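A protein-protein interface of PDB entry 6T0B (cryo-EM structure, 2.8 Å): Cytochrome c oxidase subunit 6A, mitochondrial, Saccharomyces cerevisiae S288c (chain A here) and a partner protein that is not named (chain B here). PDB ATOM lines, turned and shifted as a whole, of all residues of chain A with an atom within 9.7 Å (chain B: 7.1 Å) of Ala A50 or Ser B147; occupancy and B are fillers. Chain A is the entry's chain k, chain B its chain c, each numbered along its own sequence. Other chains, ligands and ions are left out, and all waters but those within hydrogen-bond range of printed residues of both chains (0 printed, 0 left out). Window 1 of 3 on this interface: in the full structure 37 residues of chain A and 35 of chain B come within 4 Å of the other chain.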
ATOM      1  N   TRP A  42      -6.247 -15.467  21.547  1.00  0.00           N
ATOM      2  CA  TRP A  42      -7.221 -14.502  21.055  1.00  0.00           C
ATOM      3  C   TRP A  42      -6.628 -13.522  20.053  1.00  0.00           C
ATOM      4  O   TRP A  42      -7.344 -13.075  19.155  1.00  0.00           O
ATOM      5  CB  TRP A  42      -7.868 -13.753  22.214  1.00  0.00           C
ATOM      6  CG  TRP A  42      -9.101 -14.428  22.711  1.00  0.00           C
ATOM      7  CD1 TRP A  42      -9.273 -15.013  23.922  1.00  0.00           C
ATOM      8  CD2 TRP A  42     -10.329 -14.605  22.004  1.00  0.00           C
ATOM      9  NE1 TRP A  42     -10.534 -15.539  24.023  1.00  0.00           N
ATOM     10  CE2 TRP A  42     -11.203 -15.298  22.854  1.00  0.00           C
ATOM     11  CE3 TRP A  42     -10.779 -14.232  20.739  1.00  0.00           C
ATOM     12  CZ2 TRP A  42     -12.491 -15.634  22.477  1.00  0.00           C
ATOM     13  CZ3 TRP A  42     -12.057 -14.564  20.373  1.00  0.00           C
ATOM     14  CH2 TRP A  42     -12.899 -15.252  21.237  1.00  0.00           C
ATOM     15  N   VAL A  43      -5.338 -13.183  20.161  1.00  0.00           N
ATOM     16  CA  VAL A  43      -4.701 -12.445  19.069  1.00  0.00           C
ATOM     17  C   VAL A  43      -4.579 -13.344  17.840  1.00  0.00           C
ATOM     18  O   VAL A  43      -4.734 -12.875  16.698  1.00  0.00           O
ATOM     19  CB  VAL A  43      -3.339 -11.873  19.514  1.00  0.00           C
ATOM     20  CG1 VAL A  43      -2.581 -11.219  18.358  1.00  0.00           C
ATOM     21  CG2 VAL A  43      -3.514 -10.897  20.644  1.00  0.00           C
ATOM     22  N   LYS A  44      -4.355 -14.649  18.058  1.00  0.00           N
ATOM     23  CA  LYS A  44      -4.373 -15.614  16.962  1.00  0.00           C
ATOM     24  C   LYS A  44      -5.719 -15.617  16.245  1.00  0.00           C
ATOM     25  O   LYS A  44      -5.772 -15.566  15.011  1.00  0.00           O
ATOM     26  CB  LYS A  44      -4.042 -17.007  17.494  1.00  0.00           C
ATOM     27  CG  LYS A  44      -3.279 -17.875  16.516  1.00  0.00           C
ATOM     28  CD  LYS A  44      -3.279 -19.330  16.936  1.00  0.00           C
ATOM     29  CE  LYS A  44      -2.635 -20.201  15.869  1.00  0.00           C
ATOM     30  NZ  LYS A  44      -2.905 -21.650  16.081  1.00  0.00           N
ATOM     31  N   ILE A  45      -6.815 -15.599  17.006  1.00  0.00           N
ATOM     32  CA  ILE A  45      -8.142 -15.553  16.396  1.00  0.00           C
ATOM     33  C   ILE A  45      -8.391 -14.200  15.726  1.00  0.00           C
ATOM     34  O   ILE A  45      -8.871 -14.139  14.585  1.00  0.00           O
ATOM     35  CB  ILE A  45      -9.219 -15.891  17.445  1.00  0.00           C
ATOM     36  CG1 ILE A  45      -9.185 -17.386  17.772  1.00  0.00           C
ATOM     37  CG2 ILE A  45     -10.611 -15.505  16.967  1.00  0.00           C
ATOM     38  CD1 ILE A  45     -10.187 -17.808  18.811  1.00  0.00           C
ATOM     39  N   SER A  46      -8.007 -13.101  16.388  1.00  0.00           N
ATOM     40  CA  SER A  46      -8.273 -11.753  15.899  1.00  0.00           C
ATOM     41  C   SER A  46      -7.472 -11.387  14.663  1.00  0.00           C
ATOM     42  O   SER A  46      -7.814 -10.403  14.003  1.00  0.00           O
ATOM     43  CB  SER A  46      -7.970 -10.709  16.970  1.00  0.00           C
ATOM     44  OG  SER A  46      -6.582 -10.526  17.123  1.00  0.00           O
ATOM     45  N   VAL A  47      -6.386 -12.095  14.364  1.00  0.00           N
ATOM     46  CA  VAL A  47      -5.657 -11.848  13.133  1.00  0.00           C
ATOM     47  C   VAL A  47      -5.872 -12.948  12.091  1.00  0.00           C
ATOM     48  O   VAL A  47      -5.699 -12.687  10.896  1.00  0.00           O
ATOM     49  CB  VAL A  47      -4.153 -11.621  13.406  1.00  0.00           C
ATOM     50  CG1 VAL A  47      -3.408 -12.928  13.579  1.00  0.00           C
ATOM     51  CG2 VAL A  47      -3.520 -10.758  12.326  1.00  0.00           C
ATOM     52  N   TRP A  48      -6.288 -14.155  12.487  1.00  0.00           N
ATOM     53  CA  TRP A  48      -6.524 -15.172  11.473  1.00  0.00           C
ATOM     54  C   TRP A  48      -7.937 -15.108  10.918  1.00  0.00           C
ATOM     55  O   TRP A  48      -8.171 -15.569   9.797  1.00  0.00           O
ATOM     56  CB  TRP A  48      -6.271 -16.574  12.033  1.00  0.00           C
ATOM     57  CG  TRP A  48      -4.834 -17.037  12.062  1.00  0.00           C
ATOM     58  CD1 TRP A  48      -4.121 -17.395  13.164  1.00  0.00           C
ATOM     59  CD2 TRP A  48      -3.955 -17.225  10.944  1.00  0.00           C
ATOM     60  NE1 TRP A  48      -2.854 -17.777  12.813  1.00  0.00           N
ATOM     61  CE2 TRP A  48      -2.725 -17.682  11.453  1.00  0.00           C
ATOM     62  CE3 TRP A  48      -4.084 -17.044   9.565  1.00  0.00           C
ATOM     63  CZ2 TRP A  48      -1.635 -17.960  10.637  1.00  0.00           C
ATOM     64  CZ3 TRP A  48      -3.001 -17.320   8.757  1.00  0.00           C
ATOM     65  CH2 TRP A  48      -1.792 -17.774   9.295  1.00  0.00           C
ATOM     66  N   VAL A  49      -8.892 -14.577  11.676  1.00  0.00           N
ATOM     67  CA  VAL A  49     -10.293 -14.596  11.286  1.00  0.00           C
ATOM     68  C   VAL A  49     -10.846 -13.190  11.084  1.00  0.00           C
ATOM     69  O   VAL A  49     -11.548 -12.934  10.103  1.00  0.00           O
ATOM     70  CB  VAL A  49     -11.140 -15.380  12.315  1.00  0.00           C
ATOM     71  CG1 VAL A  49     -12.596 -15.447  11.888  1.00  0.00           C
ATOM     72  CG2 VAL A  49     -10.591 -16.782  12.507  1.00  0.00           C
ATOM     73  N   ALA A  50     -10.516 -12.255  11.978  1.00  0.00           N
ATOM     74  CA  ALA A  50     -11.165 -10.948  11.946  1.00  0.00           C
ATOM     75  C   ALA A  50     -10.625 -10.054  10.836  1.00  0.00           C
ATOM     76  O   ALA A  50     -11.392  -9.315  10.210  1.00  0.00           O
ATOM     77  CB  ALA A  50     -11.028 -10.264  13.303  1.00  0.00           C
ATOM     78  N   LEU A  51      -9.327 -10.092  10.575  1.00  0.00           N
ATOM     79  CA  LEU A  51      -8.794  -9.296   9.472  1.00  0.00           C
ATOM     80  C   LEU A  51      -8.920  -9.968   8.101  1.00  0.00           C
ATOM     81  O   LEU A  51      -8.995  -9.252   7.093  1.00  0.00           O
ATOM     82  CB  LEU A  51      -7.350  -8.876   9.754  1.00  0.00           C
ATOM     83  CG  LEU A  51      -7.214  -7.548  10.529  1.00  0.00           C
ATOM     84  CD1 LEU A  51      -7.951  -6.440   9.775  1.00  0.00           C
ATOM     85  CD2 LEU A  51      -7.647  -7.606  11.997  1.00  0.00           C
ATOM     86  N   PRO A  52      -8.967 -11.320   7.988  1.00  0.00           N
ATOM     87  CA  PRO A  52      -9.520 -11.911   6.758  1.00  0.00           C
ATOM     88  C   PRO A  52     -11.038 -11.865   6.636  1.00  0.00           C
ATOM     89  O   PRO A  52     -11.607 -12.574   5.804  1.00  0.00           O
ATOM     90  CB  PRO A  52      -9.027 -13.361   6.820  1.00  0.00           C
ATOM     91  CG  PRO A  52      -7.758 -13.252   7.512  1.00  0.00           C
ATOM     92  CD  PRO A  52      -8.041 -12.281   8.619  1.00  0.00           C
ATOM     93  N   ALA A  53     -11.706 -11.070   7.466  1.00  0.00           N
ATOM     94  CA  ALA A  53     -13.102 -10.725   7.269  1.00  0.00           C
ATOM     95  C   ALA A  53     -13.260  -9.300   6.767  1.00  0.00           C
ATOM     96  O   ALA A  53     -14.008  -9.048   5.812  1.00  0.00           O
ATOM     97  CB  ALA A  53     -13.879 -10.918   8.575  1.00  0.00           C
ATOM     98  N   ILE A  54     -12.550  -8.359   7.392  1.00  0.00           N
ATOM     99  CA  ILE A  54     -12.526  -6.987   6.904  1.00  0.00           C
ATOM    100  C   ILE A  54     -11.835  -6.924   5.549  1.00  0.00           C
ATOM    101  O   ILE A  54     -12.238  -6.146   4.677  1.00  0.00           O
ATOM    102  CB  ILE A  54     -11.852  -6.069   7.941  1.00  0.00           C
ATOM    103  CG1 ILE A  54     -12.501  -6.258   9.310  1.00  0.00           C
ATOM    104  CG2 ILE A  54     -11.934  -4.603   7.521  1.00  0.00           C
ATOM    105  CD1 ILE A  54     -11.940  -5.360  10.380  1.00  0.00           C
ATOM    106  N   ALA A  55     -10.834  -7.781   5.327  1.00  0.00           N
ATOM    107  CA  ALA A  55     -10.165  -7.846   4.036  1.00  0.00           C
ATOM    108  C   ALA A  55     -11.073  -8.347   2.916  1.00  0.00           C
ATOM    109  O   ALA A  55     -10.837  -8.002   1.754  1.00  0.00           O
ATOM    110  CB  ALA A  55      -8.928  -8.736   4.136  1.00  0.00           C
ATOM    111  N   LEU A  56     -12.097  -9.147   3.225  1.00  0.00           N
ATOM    112  CA  LEU A  56     -13.021  -9.581   2.185  1.00  0.00           C
ATOM    113  C   LEU A  56     -14.269  -8.716   2.085  1.00  0.00           C
ATOM    114  O   LEU A  56     -14.958  -8.779   1.062  1.00  0.00           O
ATOM    115  CB  LEU A  56     -13.439 -11.051   2.378  1.00  0.00           C
ATOM    116  CG  LEU A  56     -14.197 -11.676   3.559  1.00  0.00           C
ATOM    117  CD1 LEU A  56     -15.713 -11.478   3.516  1.00  0.00           C
ATOM    118  CD2 LEU A  56     -13.909 -13.162   3.546  1.00  0.00           C
ATOM    119  N   THR A  57     -14.604  -7.948   3.121  1.00  0.00           N
ATOM    120  CA  THR A  57     -15.781  -7.094   3.031  1.00  0.00           C
ATOM    121  C   THR A  57     -15.451  -5.674   2.584  1.00  0.00           C
ATOM    122  O   THR A  57     -16.324  -4.994   2.033  1.00  0.00           O
ATOM    123  CB  THR A  57     -16.522  -7.087   4.372  1.00  0.00           C
ATOM    124  OG1 THR A  57     -16.514  -8.414   4.911  1.00  0.00           O
ATOM    125  CG2 THR A  57     -17.973  -6.670   4.202  1.00  0.00           C
ATOM    126  N   ALA A  58     -14.206  -5.218   2.754  1.00  0.00           N
ATOM    127  CA  ALA A  58     -13.832  -3.914   2.213  1.00  0.00           C
ATOM    128  C   ALA A  58     -13.806  -3.938   0.690  1.00  0.00           C
ATOM    129  O   ALA A  58     -14.227  -2.973   0.040  1.00  0.00           O
ATOM    130  CB  ALA A  58     -12.477  -3.480   2.769  1.00  0.00           C
ATOM    131  N   LEU B 140     -20.538  -5.148   6.851  1.00  0.00           N
ATOM    132  CA  LEU B 140     -19.286  -4.635   7.392  1.00  0.00           C
ATOM    133  C   LEU B 140     -19.468  -4.125   8.815  1.00  0.00           C
ATOM    134  O   LEU B 140     -18.559  -4.242   9.642  1.00  0.00           O
ATOM    135  CB  LEU B 140     -18.744  -3.531   6.491  1.00  0.00           C
ATOM    136  CG  LEU B 140     -17.427  -2.883   6.916  1.00  0.00           C
ATOM    137  CD1 LEU B 140     -16.308  -3.910   6.939  1.00  0.00           C
ATOM    138  CD2 LEU B 140     -17.069  -1.721   6.021  1.00  0.00           C
ATOM    139  N   THR B 142     -21.565  -5.465  10.996  1.00  0.00           N
ATOM    140  CA  THR B 142     -21.548  -6.629  11.876  1.00  0.00           C
ATOM    141  C   THR B 142     -20.135  -7.167  12.037  1.00  0.00           C
ATOM    142  O   THR B 142     -19.770  -7.651  13.117  1.00  0.00           O
ATOM    143  CB  THR B 142     -22.441  -7.744  11.352  1.00  0.00           C
ATOM    144  OG1 THR B 142     -21.969  -8.168  10.071  1.00  0.00           O
ATOM    145  CG2 THR B 142     -23.860  -7.307  11.249  1.00  0.00           C
ATOM    146  N   ILE B 143     -19.340  -7.095  10.970  1.00  0.00           N
ATOM    147  CA  ILE B 143     -17.989  -7.638  11.017  1.00  0.00           C
ATOM    148  C   ILE B 143     -17.109  -6.816  11.948  1.00  0.00           C
ATOM    149  O   ILE B 143     -16.388  -7.367  12.786  1.00  0.00           O
ATOM    150  CB  ILE B 143     -17.414  -7.725   9.596  1.00  0.00           C
ATOM    151  CG1 ILE B 143     -18.077  -8.870   8.837  1.00  0.00           C
ATOM    152  CG2 ILE B 143     -15.929  -7.941   9.623  1.00  0.00           C
ATOM    153  CD1 ILE B 143     -18.060 -10.196   9.562  1.00  0.00           C
ATOM    154  N   ILE B 144     -17.207  -5.486  11.879  1.00  0.00           N
ATOM    155  CA  ILE B 144     -16.391  -4.639  12.746  1.00  0.00           C
ATOM    156  C   ILE B 144     -16.940  -4.528  14.153  1.00  0.00           C
ATOM    157  O   ILE B 144     -16.364  -3.802  14.972  1.00  0.00           O
ATOM    158  CB  ILE B 144     -16.207  -3.221  12.176  1.00  0.00           C
ATOM    159  CG1 ILE B 144     -17.525  -2.465  12.188  1.00  0.00           C
ATOM    160  CG2 ILE B 144     -15.586  -3.287  10.792  1.00  0.00           C
ATOM    161  CD1 ILE B 144     -17.511  -1.213  11.353  1.00  0.00           C
ATOM    162  N   LEU B 145     -18.026  -5.220  14.470  1.00  0.00           N
ATOM    163  CA  LEU B 145     -18.465  -5.350  15.851  1.00  0.00           C
ATOM    164  C   LEU B 145     -18.087  -6.695  16.447  1.00  0.00           C
ATOM    165  O   LEU B 145     -17.600  -6.755  17.589  1.00  0.00           O
ATOM    166  CB  LEU B 145     -19.974  -5.147  15.956  1.00  0.00           C
ATOM    167  CG  LEU B 145     -20.409  -3.764  16.432  1.00  0.00           C
ATOM    168  CD1 LEU B 145     -19.854  -2.663  15.559  1.00  0.00           C
ATOM    169  CD2 LEU B 145     -21.902  -3.698  16.465  1.00  0.00           C
ATOM    170  N   LEU B 146     -18.265  -7.771  15.675  1.00  0.00           N
ATOM    171  CA  LEU B 146     -17.757  -9.072  16.086  1.00  0.00           C
ATOM    172  C   LEU B 146     -16.239  -9.075  16.200  1.00  0.00           C
ATOM    173  O   LEU B 146     -15.682  -9.845  16.988  1.00  0.00           O
ATOM    174  CB  LEU B 146     -18.207 -10.149  15.106  1.00  0.00           C
ATOM    175  CG  LEU B 146     -19.651 -10.607  15.240  1.00  0.00           C
ATOM    176  CD1 LEU B 146     -19.956 -11.680  14.213  1.00  0.00           C
ATOM    177  CD2 LEU B 146     -19.902 -11.122  16.638  1.00  0.00           C
ATOM    178  N   SER B 147     -15.553  -8.223  15.440  1.00  0.00           N
ATOM    179  CA  SER B 147     -14.112  -8.108  15.592  1.00  0.00           C
ATOM    180  C   SER B 147     -13.732  -7.189  16.741  1.00  0.00           C
ATOM    181  O   SER B 147     -12.681  -7.386  17.357  1.00  0.00           O
ATOM    182  CB  SER B 147     -13.484  -7.594  14.303  1.00  0.00           C
ATOM    183  OG  SER B 147     -13.836  -6.244  14.087  1.00  0.00           O
ATOM    184  N   SER B 148     -14.556  -6.184  17.037  1.00  0.00           N
ATOM    185  CA  SER B 148     -14.256  -5.289  18.148  1.00  0.00           C
ATOM    186  C   SER B 148     -14.354  -6.020  19.471  1.00  0.00           C
ATOM    187  O   SER B 148     -13.560  -5.771  20.391  1.00  0.00           O
ATOM    188  CB  SER B 148     -15.204  -4.099  18.142  1.00  0.00           C
ATOM    189  OG  SER B 148     -16.518  -4.510  18.463  1.00  0.00           O
ATOM    190  N   GLY B 149     -15.308  -6.944  19.570  1.00  0.00           N
ATOM    191  CA  GLY B 149     -15.364  -7.803  20.739  1.00  0.00           C
ATOM    192  C   GLY B 149     -14.142  -8.694  20.873  1.00  0.00           C
ATOM    193  O   GLY B 149     -13.634  -8.906  21.977  1.00  0.00           O
ATOM    194  N   ALA B 150     -13.636  -9.201  19.751  1.00  0.00           N
ATOM    195  CA  ALA B 150     -12.449 -10.045  19.793  1.00  0.00           C
ATOM    196  C   ALA B 150     -11.208  -9.252  20.155  1.00  0.00           C
ATOM    197  O   ALA B 150     -10.272  -9.802  20.741  1.00  0.00           O
ATOM    198  CB  ALA B 150     -12.246 -10.742  18.453  1.00  0.00           C
ATOM    199  N   THR B 151     -11.176  -7.970  19.806  1.00  0.00           N
ATOM    200  CA  THR B 151     -10.049  -7.140  20.210  1.00  0.00           C
ATOM    201  C   THR B 151     -10.097  -6.840  21.694  1.00  0.00           C
ATOM    202  O   THR B 151      -9.082  -6.955  22.390  1.00  0.00           O
ATOM    203  CB  THR B 151     -10.020  -5.842  19.421  1.00  0.00           C
ATOM    204  OG1 THR B 151     -11.272  -5.167  19.568  1.00  0.00           O
ATOM    205  CG2 THR B 151      -9.748  -6.118  17.970  1.00  0.00           C
ATOM    206  N   VAL B 152     -11.271  -6.450  22.197  1.00  0.00           N
ATOM    207  CA  VAL B 152     -11.370  -6.077  23.601  1.00  0.00           C
ATOM    208  C   VAL B 152     -11.218  -7.291  24.510  1.00  0.00           C
ATOM    209  O   VAL B 152     -10.761  -7.142  25.649  1.00  0.00           O
ATOM    210  CB  VAL B 152     -12.682  -5.312  23.868  1.00  0.00           C
ATOM    211  CG1 VAL B 152     -13.893  -6.227  23.829  1.00  0.00           C
ATOM    212  CG2 VAL B 152     -12.612  -4.529  25.175  1.00  0.00           C
ATOM    213  N   THR B 153     -11.486  -8.502  24.009  1.00  0.00           N
ATOM    214  CA  THR B 153     -11.252  -9.694  24.817  1.00  0.00           C
ATOM    215  C   THR B 153      -9.763  -9.930  25.052  1.00  0.00           C
ATOM    216  O   THR B 153      -9.345 -10.185  26.190  1.00  0.00           O
ATOM    217  CB  THR B 153     -11.902 -10.909  24.161  1.00  0.00           C
ATOM    218  OG1 THR B 153     -13.312 -10.697  24.058  1.00  0.00           O
ATOM    219  CG2 THR B 153     -11.678 -12.143  24.991  1.00  0.00           C
ATOM    220  N   TYR B 154      -8.933  -9.817  24.010  1.00  0.00           N
ATOM    221  CA  TYR B 154      -7.505 -10.004  24.255  1.00  0.00           C
ATOM    222  C   TYR B 154      -6.896  -8.806  24.951  1.00  0.00           C
ATOM    223  O   TYR B 154      -5.897  -8.962  25.652  1.00  0.00           O
ATOM    224  CB  TYR B 154      -6.725 -10.347  22.972  1.00  0.00           C
ATOM    225  CG  TYR B 154      -6.397  -9.272  21.934  1.00  0.00           C
ATOM    226  CD1 TYR B 154      -5.391  -8.329  22.129  1.00  0.00           C
ATOM    227  CD2 TYR B 154      -7.034  -9.276  20.705  1.00  0.00           C
ATOM    228  CE1 TYR B 154      -5.084  -7.390  21.165  1.00  0.00           C
ATOM    229  CE2 TYR B 154      -6.725  -8.341  19.729  1.00  0.00           C
ATOM    230  CZ  TYR B 154      -5.753  -7.402  19.970  1.00  0.00           C
ATOM    231  OH  TYR B 154      -5.454  -6.468  19.004  1.00  0.00           O
ATOM    232  N   ILE B 173      -7.380  -0.341  19.187  1.00  0.00           N
ATOM    233  CA  ILE B 173      -8.023  -0.940  18.024  1.00  0.00           C
ATOM    234  C   ILE B 173      -9.521  -1.050  18.247  1.00  0.00           C
ATOM    235  O   ILE B 173     -10.312  -0.788  17.336  1.00  0.00           O
ATOM    236  CB  ILE B 173      -7.378  -2.299  17.714  1.00  0.00           C
ATOM    237  CG1 ILE B 173      -5.966  -2.098  17.200  1.00  0.00           C
ATOM    238  CG2 ILE B 173      -8.123  -3.030  16.642  1.00  0.00           C
ATOM    239  CD1 ILE B 173      -5.141  -3.343  17.243  1.00  0.00           C
ATOM    240  N   THR B 174      -9.933  -1.375  19.476  1.00  0.00           N
ATOM    241  CA  THR B 174     -11.355  -1.454  19.798  1.00  0.00           C
ATOM    242  C   THR B 174     -12.028  -0.098  19.664  1.00  0.00           C
ATOM    243  O   THR B 174     -13.106   0.014  19.066  1.00  0.00           O
ATOM    244  CB  THR B 174     -11.535  -1.991  21.207  1.00  0.00           C
ATOM    245  OG1 THR B 174     -10.912  -3.273  21.308  1.00  0.00           O
ATOM    246  CG2 THR B 174     -12.988  -2.125  21.543  1.00  0.00           C
ATOM    247  N   LEU B 177     -12.250   0.913  15.973  1.00  0.00           N
ATOM    248  CA  LEU B 177     -13.279   0.152  15.274  1.00  0.00           C
ATOM    249  C   LEU B 177     -14.680   0.613  15.645  1.00  0.00           C
ATOM    250  O   LEU B 177     -15.581   0.610  14.789  1.00  0.00           O
ATOM    251  CB  LEU B 177     -13.123  -1.332  15.567  1.00  0.00           C
ATOM    252  CG  LEU B 177     -12.020  -2.030  14.783  1.00  0.00           C
ATOM    253  CD1 LEU B 177     -12.146  -3.524  14.933  1.00  0.00           C
ATOM    254  CD2 LEU B 177     -12.049  -1.645  13.317  1.00  0.00           C
ATOM    255  N   ASP B 254     -23.236  -5.750  21.041  1.00  0.00           N
ATOM    256  CA  ASP B 254     -23.004  -6.668  19.933  1.00  0.00           C
ATOM    257  C   ASP B 254     -24.227  -7.533  19.661  1.00  0.00           C
ATOM    258  O   ASP B 254     -24.674  -7.651  18.515  1.00  0.00           O
ATOM    259  CB  ASP B 254     -21.791  -7.532  20.254  1.00  0.00           C
ATOM    260  CG  ASP B 254     -21.451  -8.503  19.155  1.00  0.00           C
ATOM    261  OD1 ASP B 254     -21.739  -8.216  17.976  1.00  0.00           O
ATOM    262  OD2 ASP B 254     -20.878  -9.565  19.479  1.00  0.00           O
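OG1 of Thr B151 sits close to O of Ser B147, 3.4 Å away. The side-chain hydroxyl (OG) of Ser A46 is in hydrogen-bond range of the backbone carbonyl oxygen (O) of Val A43 (3.0 Å). O of Ala A53 lies within hydrogen-bond range of OG1 of Thr A57 (2.7 Å). O of Ile B143 lies within hydrogen-bond range of OG of Ser B147. The backbone carbonyl oxygen (O) of Gly B149 is in hydrogen-bond range of the side-chain hydroxyl (OG1) of Thr B153, 2.8 Å away. O of Trp A42 sits close to OG of Ser A46 (3.3 Å).
Among the printed residues, pairs that only touch across the chains: Ser A46 with Tyr B154, Val A43 with Tyr B154, Trp A42 with Tyr B154, Trp A42 with Thr B153, Ala A50 with Ser B147, Ala A53 with Ile B143, Ile A54 with Ile B143 and Thr A57 with Leu B140.
Ala A50 touches just one residue of chain B: Ser B147. Of chain A, only Ala A50 comes within 4 Å of Ser B147. No residue of chain A comes within 4 Å of Ser B148. Gly B149 touches none of the printed residues of chain A. No residue of chain A comes within 4 Å of Ala B150. Printed residues of chain A within 4 Å of Leu B140: Thr A57 (3.96 Å). Printed residues of chain A within 4 Å of Thr B153: Trp A42. Leu A56 touches none of the printed residues of chain B. The nearest residue of chain B that does not touch Ala A50 is Ile B143 (4.8 Å). The nearest residue of chain A that does not touch Ser B147 is Ile A54 (4.3 Å).
Of the 17 printed residues of chain A, 7 touch a printed residue of chain B. Printed residues of chain A that touch a printed residue of chain B: Trp A42, Val A43, Ser A46, Ala A50, Ala A53, Ile A54 and Thr A57. Hydrophobic or aromatic side chains of chain A within 4 Å of the printed part of chain B: Trp A42, Val A43, Ala A50, Ala A53 and Ile A54. Of the 18 printed residues of chain B, 5 touch a printed residue of chain A. Among the printed residues, no Asp or Glu carboxylate lies within 4 Å of a Lys or Arg side-chain nitrogen of the other chain.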
